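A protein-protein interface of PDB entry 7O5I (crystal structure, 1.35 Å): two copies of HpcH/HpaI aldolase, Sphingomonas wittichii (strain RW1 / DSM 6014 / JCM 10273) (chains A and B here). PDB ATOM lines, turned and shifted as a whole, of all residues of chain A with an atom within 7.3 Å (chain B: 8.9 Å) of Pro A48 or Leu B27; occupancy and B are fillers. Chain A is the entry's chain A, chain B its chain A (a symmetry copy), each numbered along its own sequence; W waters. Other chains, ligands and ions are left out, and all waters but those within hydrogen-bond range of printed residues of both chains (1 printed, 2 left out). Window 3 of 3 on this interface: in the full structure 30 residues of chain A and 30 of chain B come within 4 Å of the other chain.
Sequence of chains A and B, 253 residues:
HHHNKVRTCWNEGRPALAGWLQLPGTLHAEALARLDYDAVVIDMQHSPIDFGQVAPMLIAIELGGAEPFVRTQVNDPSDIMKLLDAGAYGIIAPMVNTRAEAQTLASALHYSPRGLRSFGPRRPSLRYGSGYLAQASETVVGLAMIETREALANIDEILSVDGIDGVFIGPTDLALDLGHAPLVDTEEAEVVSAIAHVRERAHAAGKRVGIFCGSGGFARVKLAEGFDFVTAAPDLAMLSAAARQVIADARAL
The side-chain carboxylate (OD2) of Asp A235 is in hydrogen-bond range of the backbone NH (N) of Leu A23 (3.1 Å).
The backbone carbonyl oxygen (O) of Pro A48 sits at hydrogen-bond distance from the side-chain amide nitrogen (NE2) of Gln A53, at 3.4 Å.
The side-chain hydroxyl (OG) of Ser A240 is in hydrogen-bond range of the backbone carbonyl oxygen (O) of Leu A236.
O of Leu B23 is in hydrogen-bond range of NE2 of His B28, 2.9 Å away.
Among the printed residues, pairs that only touch across the chains: Pro A24 with Pro B24, Leu A236 with Leu B27, Leu A23 with His B28, Pro A48 with Leu B27 and Leu A23 with Leu B27.
Leu B27 touches three residues of chain A.
No residue of chain B comes within 4 Å of Ser A47.
Printed residues of chain A within 4 Å of His B28: Leu A23 (3.8 Å).
Of the printed residues of chain B, Leu A236 touches Leu B27 (3.7 Å).
Of the printed residues of chain A, Pro B24 touches Pro A24 (3.7 Å).
Of the printed residues of chain B, Leu A23 touches Leu B27 (3.96 Å) and His B28 (3.8 Å).
Of the printed residues of chain B, Pro A24 touches Pro B24 (3.7 Å).
Leu B32 touches none of the printed residues of chain A.
Arg B34 touches none of the printed residues of chain A.
The nearest residue of chain A that does not touch Leu B27 is Gln A22 (4.3 Å).
Of the 16 printed residues of chain A, 4 touch a printed residue of chain B.
Hydrophobic or aromatic side chains of chain A within 4 Å of the printed part of chain B: Leu A23, Pro A48 and Leu A236.
Along chain A the printed residues that touch a printed residue of chain B span positions 23 to 236.
Hydrophobic or aromatic side chains of chain B that line the printed part of chain A: Leu B27 and His B28.
Among the printed residues, 5 pairs touch across the chains.
Among the printed residues, no Asp or Glu carboxylate lies within 4 Å of a Lys or Arg side-chain nitrogen of the other chain.
Pro B24 touches its own counterpart, Pro A24.
2 positions are printed for both chains.
Water W1 lies within hydrogen-bond range of O of Pro A24 (3.2 Å) and O of Pro B24 (3.2 Å).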
ATOM      1  N   GLN A  22     -11.194  -3.482  15.045  1.00  0.00           N
ATOM      2  CA  GLN A  22     -11.826  -3.355  13.747  1.00  0.00           C
ATOM      3  C   GLN A  22     -13.275  -2.899  13.835  1.00  0.00           C
ATOM      4  O   GLN A  22     -13.871  -2.597  12.805  1.00  0.00           O
ATOM      5  CB  GLN A  22     -11.737  -4.669  12.975  1.00  0.00           C
ATOM      6  CG  GLN A  22     -10.313  -4.958  12.575  1.00  0.00           C
ATOM      7  CD  GLN A  22     -10.053  -6.385  12.323  1.00  0.00           C
ATOM      8  OE1 GLN A  22     -10.862  -7.280  12.601  1.00  0.00           O
ATOM      9  NE2 GLN A  22      -8.880  -6.635  11.798  1.00  0.00           N
ATOM     10  N   LEU A  23     -13.831  -2.791  15.030  1.00  0.00           N
ATOM     11  CA  LEU A  23     -15.196  -2.335  15.221  1.00  0.00           C
ATOM     12  C   LEU A  23     -15.201  -0.869  15.598  1.00  0.00           C
ATOM     13  O   LEU A  23     -14.540  -0.476  16.576  1.00  0.00           O
ATOM     14  CB  LEU A  23     -15.889  -3.167  16.294  1.00  0.00           C
ATOM     15  CG  LEU A  23     -15.972  -4.661  16.012  1.00  0.00           C
ATOM     16  CD1 LEU A  23     -16.535  -5.398  17.242  1.00  0.00           C
ATOM     17  CD2 LEU A  23     -16.805  -4.967  14.777  1.00  0.00           C
ATOM     18  N   PRO A  24     -15.955  -0.042  14.886  1.00  0.00           N
ATOM     19  CA  PRO A  24     -16.031   1.368  15.265  1.00  0.00           C
ATOM     20  C   PRO A  24     -16.771   1.544  16.576  1.00  0.00           C
ATOM     21  O   PRO A  24     -17.617   0.739  16.935  1.00  0.00           O
ATOM     22  CB  PRO A  24     -16.798   2.022  14.115  1.00  0.00           C
ATOM     23  CG  PRO A  24     -17.539   0.919  13.430  1.00  0.00           C
ATOM     24  CD  PRO A  24     -16.680  -0.325  13.633  1.00  0.00           C
ATOM     25  N   ASP A  43      -7.674  -0.269  13.599  1.00  0.00           N
ATOM     26  CA  ASP A  43      -7.406  -0.697  12.233  1.00  0.00           C
ATOM     27  C   ASP A  43      -8.295   0.090  11.287  1.00  0.00           C
ATOM     28  O   ASP A  43      -9.523  -0.004  11.356  1.00  0.00           O
ATOM     29  CB  ASP A  43      -7.664  -2.191  12.160  1.00  0.00           C
ATOM     30  CG  ASP A  43      -7.288  -2.822  10.856  1.00  0.00           C
ATOM     31  OD1 ASP A  43      -6.951  -2.116   9.875  1.00  0.00           O
ATOM     32  OD2 ASP A  43      -7.293  -4.082  10.862  1.00  0.00           O
ATOM     33  N   MET A  44      -7.671   0.913  10.437  1.00  0.00           N
ATOM     34  CA  MET A  44      -8.389   1.651   9.396  1.00  0.00           C
ATOM     35  C   MET A  44      -8.176   1.063   8.012  1.00  0.00           C
ATOM     36  O   MET A  44      -8.630   1.646   7.022  1.00  0.00           O
ATOM     37  CB  MET A  44      -8.025   3.131   9.363  1.00  0.00           C
ATOM     38  CG  MET A  44      -8.357   3.872  10.642  1.00  0.00           C
ATOM     39  SD  MET A  44      -8.000   5.634  10.603  1.00  0.00           S
ATOM     40  CE  MET A  44      -9.284   6.245   9.536  1.00  0.00           C
ATOM     41  N   GLN A  45      -7.568  -0.112   7.920  1.00  0.00           N
ATOM     42  CA  GLN A  45      -7.368  -0.775   6.641  1.00  0.00           C
ATOM     43  C   GLN A  45      -8.420  -1.859   6.423  1.00  0.00           C
ATOM     44  O   GLN A  45      -9.178  -1.821   5.464  1.00  0.00           O
ATOM     45  CB  GLN A  45      -5.943  -1.358   6.562  1.00  0.00           C
ATOM     46  CG  GLN A  45      -5.612  -1.928   5.187  1.00  0.00           C
ATOM     47  CD  GLN A  45      -4.313  -2.681   5.185  1.00  0.00           C
ATOM     48  OE1 GLN A  45      -3.891  -3.201   6.217  1.00  0.00           O
ATOM     49  NE2 GLN A  45      -3.683  -2.774   4.025  1.00  0.00           N
ATOM     50  N   HIS A  46      -8.458  -2.847   7.297  1.00  0.00           N
ATOM     51  CA  HIS A  46      -9.356  -3.992   7.151  1.00  0.00           C
ATOM     52  C   HIS A  46     -10.510  -3.883   8.131  1.00  0.00           C
ATOM     53  O   HIS A  46     -10.687  -4.721   9.028  1.00  0.00           O
ATOM     54  CB  HIS A  46      -8.588  -5.295   7.285  1.00  0.00           C
ATOM     55  CG  HIS A  46      -7.612  -5.510   6.168  1.00  0.00           C
ATOM     56  ND1 HIS A  46      -7.993  -5.630   4.843  1.00  0.00           N
ATOM     57  CD2 HIS A  46      -6.255  -5.554   6.173  1.00  0.00           C
ATOM     58  CE1 HIS A  46      -6.913  -5.789   4.094  1.00  0.00           C
ATOM     59  NE2 HIS A  46      -5.851  -5.726   4.876  1.00  0.00           N
ATOM     60  N   SER A  47     -11.268  -2.819   7.972  1.00  0.00           N
ATOM     61  CA  SER A  47     -12.386  -2.491   8.842  1.00  0.00           C
ATOM     62  C   SER A  47     -13.209  -1.438   8.142  1.00  0.00           C
ATOM     63  O   SER A  47     -12.781  -0.885   7.117  1.00  0.00           O
ATOM     64  CB  SER A  47     -11.880  -1.869  10.135  1.00  0.00           C
ATOM     65  OG  SER A  47     -11.593  -0.490   9.890  1.00  0.00           O
ATOM     66  N   PRO A  48     -14.366  -1.099   8.690  1.00  0.00           N
ATOM     67  CA  PRO A  48     -15.152   0.007   8.134  1.00  0.00           C
ATOM     68  C   PRO A  48     -14.899   1.310   8.870  1.00  0.00           C
ATOM     69  O   PRO A  48     -15.703   2.244   8.777  1.00  0.00           O
ATOM     70  CB  PRO A  48     -16.592  -0.464   8.329  1.00  0.00           C
ATOM     71  CG  PRO A  48     -16.528  -1.249   9.579  1.00  0.00           C
ATOM     72  CD  PRO A  48     -15.158  -1.934   9.610  1.00  0.00           C
ATOM     73  N   ILE A  49     -13.794   1.407   9.603  1.00  0.00           N
ATOM     74  CA  ILE A  49     -13.521   2.595  10.401  1.00  0.00           C
ATOM     75  C   ILE A  49     -12.883   3.654   9.513  1.00  0.00           C
ATOM     76  O   ILE A  49     -11.733   3.510   9.109  1.00  0.00           O
ATOM     77  CB  ILE A  49     -12.636   2.274  11.608  1.00  0.00           C
ATOM     78  CG1 ILE A  49     -13.262   1.176  12.471  1.00  0.00           C
ATOM     79  CG2 ILE A  49     -12.362   3.557  12.430  1.00  0.00           C
ATOM     80  CD1 ILE A  49     -12.370   0.715  13.596  1.00  0.00           C
ATOM     81  N   ASP A  50     -13.610   4.732   9.250  1.00  0.00           N
ATOM     82  CA  ASP A  50     -13.134   5.900   8.532  1.00  0.00           C
ATOM     83  C   ASP A  50     -12.677   6.973   9.522  1.00  0.00           C
ATOM     84  O   ASP A  50     -12.749   6.808  10.742  1.00  0.00           O
ATOM     85  CB  ASP A  50     -14.229   6.442   7.610  1.00  0.00           C
ATOM     86  CG  ASP A  50     -15.425   6.977   8.355  1.00  0.00           C
ATOM     87  OD1 ASP A  50     -15.670   6.593   9.494  1.00  0.00           O
ATOM     88  OD2 ASP A  50     -16.085   7.831   7.779  1.00  0.00           O
ATOM     89  N   PHE A  51     -12.212   8.103   8.983  1.00  0.00           N
ATOM     90  CA  PHE A  51     -11.700   9.155   9.852  1.00  0.00           C
ATOM     91  C   PHE A  51     -12.780   9.640  10.835  1.00  0.00           C
ATOM     92  O   PHE A  51     -12.512   9.844  12.026  1.00  0.00           O
ATOM     93  CB  PHE A  51     -11.149  10.332   9.039  1.00  0.00           C
ATOM     94  CG  PHE A  51     -10.462  11.339   9.919  1.00  0.00           C
ATOM     95  CD1 PHE A  51     -11.199  12.316  10.578  1.00  0.00           C
ATOM     96  CD2 PHE A  51      -9.104  11.283  10.156  1.00  0.00           C
ATOM     97  CE1 PHE A  51     -10.601  13.199  11.442  1.00  0.00           C
ATOM     98  CE2 PHE A  51      -8.516  12.144  11.023  1.00  0.00           C
ATOM     99  CZ  PHE A  51      -9.269  13.101  11.678  1.00  0.00           C
ATOM    100  N   GLN A  53     -15.158   8.153  12.222  1.00  0.00           N
ATOM    101  CA  GLN A  53     -15.305   7.235  13.337  1.00  0.00           C
ATOM    102  C   GLN A  53     -14.054   7.027  14.164  1.00  0.00           C
ATOM    103  O   GLN A  53     -14.165   6.784  15.372  1.00  0.00           O
ATOM    104  CB  GLN A  53     -15.857   5.911  12.837  1.00  0.00           C
ATOM    105  CG  GLN A  53     -17.321   6.083  12.343  1.00  0.00           C
ATOM    106  CD  GLN A  53     -17.925   4.818  11.883  1.00  0.00           C
ATOM    107  OE1 GLN A  53     -18.750   4.250  12.575  1.00  0.00           O
ATOM    108  NE2 GLN A  53     -17.570   4.380  10.692  1.00  0.00           N
ATOM    109  N   ASP A 235     -10.789  -7.266  18.152  1.00  0.00           N
ATOM    110  CA  ASP A 235     -12.086  -7.222  18.835  1.00  0.00           C
ATOM    111  C   ASP A 235     -13.119  -8.106  18.165  1.00  0.00           C
ATOM    112  O   ASP A 235     -13.768  -8.906  18.839  1.00  0.00           O
ATOM    113  CB  ASP A 235     -12.561  -5.772  19.041  1.00  0.00           C
ATOM    114  CG  ASP A 235     -12.650  -4.942  17.763  1.00  0.00           C
ATOM    115  OD1 ASP A 235     -12.331  -5.402  16.642  1.00  0.00           O
ATOM    116  OD2 ASP A 235     -13.042  -3.772  17.910  1.00  0.00           O
ATOM    117  N   LEU A 236     -13.288  -7.975  16.852  1.00  0.00           N
ATOM    118  CA  LEU A 236     -14.325  -8.730  16.163  1.00  0.00           C
ATOM    119  C   LEU A 236     -14.070 -10.229  16.293  1.00  0.00           C
ATOM    120  O   LEU A 236     -15.000 -11.002  16.535  1.00  0.00           O
ATOM    121  CB  LEU A 236     -14.386  -8.318  14.693  1.00  0.00           C
ATOM    122  CG  LEU A 236     -15.331  -9.116  13.798  1.00  0.00           C
ATOM    123  CD1 LEU A 236     -16.774  -9.085  14.305  1.00  0.00           C
ATOM    124  CD2 LEU A 236     -15.234  -8.622  12.346  1.00  0.00           C
ATOM    125  N   SER A 240     -16.666 -12.624  18.200  1.00  0.00           N
ATOM    126  CA  SER A 240     -17.280 -13.726  17.477  1.00  0.00           C
ATOM    127  C   SER A 240     -17.041 -15.035  18.206  1.00  0.00           C
ATOM    128  O   SER A 240     -17.977 -15.800  18.473  1.00  0.00           O
ATOM    129  CB  SER A 240     -16.697 -13.804  16.073  1.00  0.00           C
ATOM    130  OG  SER A 240     -17.107 -12.714  15.297  1.00  0.00           O
ATOM    131  N   LEU B  21     -26.831  -6.723  22.033  1.00  0.00           N
ATOM    132  CA  LEU B  21     -25.823  -5.763  21.584  1.00  0.00           C
ATOM    133  C   LEU B  21     -25.986  -4.425  22.289  1.00  0.00           C
ATOM    134  O   LEU B  21     -27.059  -3.810  22.244  1.00  0.00           O
ATOM    135  CB  LEU B  21     -25.902  -5.494  20.073  1.00  0.00           C
ATOM    136  CG  LEU B  21     -25.881  -6.700  19.163  1.00  0.00           C
ATOM    137  CD1 LEU B  21     -25.903  -6.247  17.693  1.00  0.00           C
ATOM    138  CD2 LEU B  21     -24.684  -7.607  19.394  1.00  0.00           C
ATOM    139  N   LEU B  23     -23.065  -2.389  21.781  1.00  0.00           N
ATOM    140  CA  LEU B  23     -22.099  -1.665  20.974  1.00  0.00           C
ATOM    141  C   LEU B  23     -22.714  -1.298  19.640  1.00  0.00           C
ATOM    142  O   LEU B  23     -23.209  -2.182  18.919  1.00  0.00           O
ATOM    143  CB  LEU B  23     -20.841  -2.503  20.772  1.00  0.00           C
ATOM    144  CG  LEU B  23     -20.116  -2.911  22.047  1.00  0.00           C
ATOM    145  CD1 LEU B  23     -18.973  -3.889  21.712  1.00  0.00           C
ATOM    146  CD2 LEU B  23     -19.585  -1.711  22.815  1.00  0.00           C
ATOM    147  N   PRO B  24     -22.668  -0.029  19.259  1.00  0.00           N
ATOM    148  CA  PRO B  24     -23.195   0.347  17.948  1.00  0.00           C
ATOM    149  C   PRO B  24     -22.329  -0.201  16.830  1.00  0.00           C
ATOM    150  O   PRO B  24     -21.139  -0.416  17.004  1.00  0.00           O
ATOM    151  CB  PRO B  24     -23.166   1.876  17.959  1.00  0.00           C
ATOM    152  CG  PRO B  24     -22.183   2.265  19.016  1.00  0.00           C
ATOM    153  CD  PRO B  24     -22.243   1.143  20.048  1.00  0.00           C
ATOM    154  N   GLY B  25     -22.929  -0.388  15.662  1.00  0.00           N
ATOM    155  CA  GLY B  25     -22.208  -0.726  14.444  1.00  0.00           C
ATOM    156  C   GLY B  25     -22.785  -1.953  13.773  1.00  0.00           C
ATOM    157  O   GLY B  25     -23.463  -2.763  14.409  1.00  0.00           O
ATOM    158  N   THR B  26     -22.542  -2.087  12.471  1.00  0.00           N
ATOM    159  CA  THR B  26     -23.118  -3.161  11.683  1.00  0.00           C
ATOM    160  C   THR B  26     -22.274  -4.414  11.570  1.00  0.00           C
ATOM    161  O   THR B  26     -22.816  -5.461  11.229  1.00  0.00           O
ATOM    162  CB  THR B  26     -23.413  -2.631  10.276  1.00  0.00           C
ATOM    163  OG1 THR B  26     -22.271  -1.949   9.767  1.00  0.00           O
ATOM    164  CG2 THR B  26     -24.562  -1.626  10.288  1.00  0.00           C
ATOM    165  N   LEU B  27     -20.959  -4.333  11.765  1.00  0.00           N
ATOM    166  CA  LEU B  27     -20.106  -5.463  11.398  1.00  0.00           C
ATOM    167  C   LEU B  27     -20.248  -6.612  12.393  1.00  0.00           C
ATOM    168  O   LEU B  27     -20.473  -7.760  12.004  1.00  0.00           O
ATOM    169  CB  LEU B  27     -18.644  -4.987  11.265  1.00  0.00           C
ATOM    170  CG  LEU B  27     -17.647  -6.096  10.896  1.00  0.00           C
ATOM    171  CD1 LEU B  27     -18.066  -6.836   9.621  1.00  0.00           C
ATOM    172  CD2 LEU B  27     -16.282  -5.456  10.689  1.00  0.00           C
ATOM    173  N   HIS B  28     -20.143  -6.322  13.690  1.00  0.00           N
ATOM    174  CA  HIS B  28     -20.396  -7.368  14.661  1.00  0.00           C
ATOM    175  C   HIS B  28     -21.858  -7.771  14.700  1.00  0.00           C
ATOM    176  O   HIS B  28     -22.163  -8.928  14.990  1.00  0.00           O
ATOM    177  CB  HIS B  28     -19.970  -6.984  16.061  1.00  0.00           C
ATOM    178  CG  HIS B  28     -20.780  -5.903  16.683  1.00  0.00           C
ATOM    179  ND1 HIS B  28     -21.048  -4.725  16.033  1.00  0.00           N
ATOM    180  CD2 HIS B  28     -21.398  -5.833  17.889  1.00  0.00           C
ATOM    181  CE1 HIS B  28     -21.803  -3.973  16.809  1.00  0.00           C
ATOM    182  NE2 HIS B  28     -22.014  -4.612  17.949  1.00  0.00           N
ATOM    183  N   ALA B  29     -22.771  -6.861  14.364  1.00  0.00           N
ATOM    184  CA  ALA B  29     -24.182  -7.218  14.319  1.00  0.00           C
ATOM    185  C   ALA B  29     -24.414  -8.311  13.286  1.00  0.00           C
ATOM    186  O   ALA B  29     -25.110  -9.295  13.564  1.00  0.00           O
ATOM    187  CB  ALA B  29     -25.008  -5.966  14.047  1.00  0.00           C
ATOM    188  N   GLU B  30     -23.879  -8.120  12.068  1.00  0.00           N
ATOM    189  CA  GLU B  30     -24.036  -9.134  11.037  1.00  0.00           C
ATOM    190  C   GLU B  30     -23.331 -10.417  11.449  1.00  0.00           C
ATOM    191  O   GLU B  30     -23.858 -11.525  11.269  1.00  0.00           O
ATOM    192  CB  GLU B  30     -23.500  -8.646   9.686  1.00  0.00           C
ATOM    193  CG  GLU B  30     -23.711  -9.663   8.536  1.00  0.00           C
ATOM    194  CD  GLU B  30     -23.082  -9.270   7.218  1.00  0.00           C
ATOM    195  OE1 GLU B  30     -22.762  -8.090   6.998  1.00  0.00           O
ATOM    196  OE2 GLU B  30     -22.901 -10.206   6.409  1.00  0.00           O
ATOM    197  N   ALA B  31     -22.100 -10.287  11.948  1.00  0.00           N
ATOM    198  CA  ALA B  31     -21.321 -11.469  12.286  1.00  0.00           C
ATOM    199  C   ALA B  31     -22.041 -12.325  13.331  1.00  0.00           C
ATOM    200  O   ALA B  31     -22.088 -13.552  13.207  1.00  0.00           O
ATOM    201  CB  ALA B  31     -19.935 -11.078  12.785  1.00  0.00           C
ATOM    202  N   LEU B  32     -22.589 -11.693  14.378  1.00  0.00           N
ATOM    203  CA  LEU B  32     -23.305 -12.447  15.404  1.00  0.00           C
ATOM    204  C   LEU B  32     -24.632 -12.986  14.887  1.00  0.00           C
ATOM    205  O   LEU B  32     -25.019 -14.105  15.246  1.00  0.00           O
ATOM    206  CB  LEU B  32     -23.499 -11.585  16.652  1.00  0.00           C
ATOM    207  CG  LEU B  32     -22.349 -11.768  17.673  1.00  0.00           C
ATOM    208  CD1 LEU B  32     -20.964 -11.564  17.063  1.00  0.00           C
ATOM    209  CD2 LEU B  32     -22.595 -10.864  18.886  1.00  0.00           C
ATOM    210  N   ALA B  33     -25.298 -12.247  14.001  1.00  0.00           N
ATOM    211  CA  ALA B  33     -26.540 -12.738  13.431  1.00  0.00           C
ATOM    212  C   ALA B  33     -26.323 -13.988  12.604  1.00  0.00           C
ATOM    213  O   ALA B  33     -27.242 -14.795  12.474  1.00  0.00           O
ATOM    214  CB  ALA B  33     -27.172 -11.638  12.598  1.00  0.00           C
ATOM    215  N   ARG B  34     -25.130 -14.146  12.019  1.00  0.00           N
ATOM    216  CA  ARG B  34     -24.847 -15.324  11.220  1.00  0.00           C
ATOM    217  C   ARG B  34     -24.519 -16.551  12.072  1.00  0.00           C
ATOM    218  O   ARG B  34     -24.456 -17.652  11.520  1.00  0.00           O
ATOM    219  CB  ARG B  34     -23.694 -15.030  10.278  1.00  0.00           C
ATOM    220  CG  ARG B  34     -24.117 -14.140   9.119  1.00  0.00           C
ATOM    221  CD  ARG B  34     -22.973 -13.826   8.187  1.00  0.00           C
ATOM    222  NE  ARG B  34     -23.332 -12.962   7.067  1.00  0.00           N
ATOM    223  CZ  ARG B  34     -23.899 -13.363   5.935  1.00  0.00           C
ATOM    224  NH1 ARG B  34     -24.244 -14.629   5.735  1.00  0.00           N
ATOM    225  NH2 ARG B  34     -24.128 -12.472   4.982  1.00  0.00           N
ATOM    226  N   PRO B  56     -29.086   1.150  10.741  1.00  0.00           N
ATOM    227  CA  PRO B  56     -28.336   0.229   9.881  1.00  0.00           C
ATOM    228  C   PRO B  56     -28.098  -1.108  10.532  1.00  0.00           C
ATOM    229  O   PRO B  56     -27.946  -2.107   9.824  1.00  0.00           O
ATOM    230  CB  PRO B  56     -27.041   1.001   9.584  1.00  0.00           C
ATOM    231  CG  PRO B  56     -26.873   1.879  10.786  1.00  0.00           C
ATOM    232  CD  PRO B  56     -28.295   2.338  11.088  1.00  0.00           C
ATOM    233  N   MET B  57     -28.063  -1.150  11.866  1.00  0.00           N
ATOM    234  CA  MET B  57     -27.883  -2.423  12.561  1.00  0.00           C
ATOM    235  C   MET B  57     -29.022  -3.384  12.310  1.00  0.00           C
ATOM    236  O   MET B  57     -28.795  -4.594  12.190  1.00  0.00           O
ATOM    237  CB  MET B  57     -27.660  -2.229  14.064  1.00  0.00           C
ATOM    238  CG  MET B  57     -26.486  -1.375  14.418  1.00  0.00           C
ATOM    239  SD  MET B  57     -26.379  -0.976  16.183  1.00  0.00           S
ATOM    240  CE  MET B  57     -25.854  -2.564  16.860  1.00  0.00           C
ATOM    241  N   ALA B  60     -28.334  -5.026   8.995  1.00  0.00           N
ATOM    242  CA  ALA B  60     -27.228  -5.967   9.070  1.00  0.00           C
ATOM    243  C   ALA B  60     -27.633  -7.273   9.743  1.00  0.00           C
ATOM    244  O   ALA B  60     -27.215  -8.344   9.305  1.00  0.00           O
ATOM    245  CB  ALA B  60     -26.077  -5.323   9.828  1.00  0.00           C
ATOM    246  N   ILE B  61     -28.446  -7.196  10.806  1.00  0.00           N
ATOM    247  CA  ILE B  61     -28.907  -8.398  11.492  1.00  0.00           C
ATOM    248  C   ILE B  61     -29.773  -9.224  10.553  1.00  0.00           C
ATOM    249  O   ILE B  61     -29.646 -10.443  10.471  1.00  0.00           O
ATOM    250  CB  ILE B  61     -29.654  -8.013  12.781  1.00  0.00           C
ATOM    251  CG1 ILE B  61     -28.626  -7.477  13.786  1.00  0.00           C
ATOM    252  CG2 ILE B  61     -30.396  -9.224  13.338  1.00  0.00           C
ATOM    253  CD1 ILE B  61     -29.283  -6.744  14.960  1.00  0.00           C
ATOM    254  N   GLY B  64     -27.709 -11.005   8.016  1.00  0.00           N
ATOM    255  CA  GLY B  64     -26.980 -12.105   8.613  1.00  0.00           C
ATOM    256  C   GLY B  64     -27.831 -13.315   8.954  1.00  0.00           C
ATOM    257  O   GLY B  64     -27.298 -14.422   9.115  1.00  0.00           O
HETATM  258  O   HOH W   1     -20.117   2.347  15.829  1.00  0.00           O
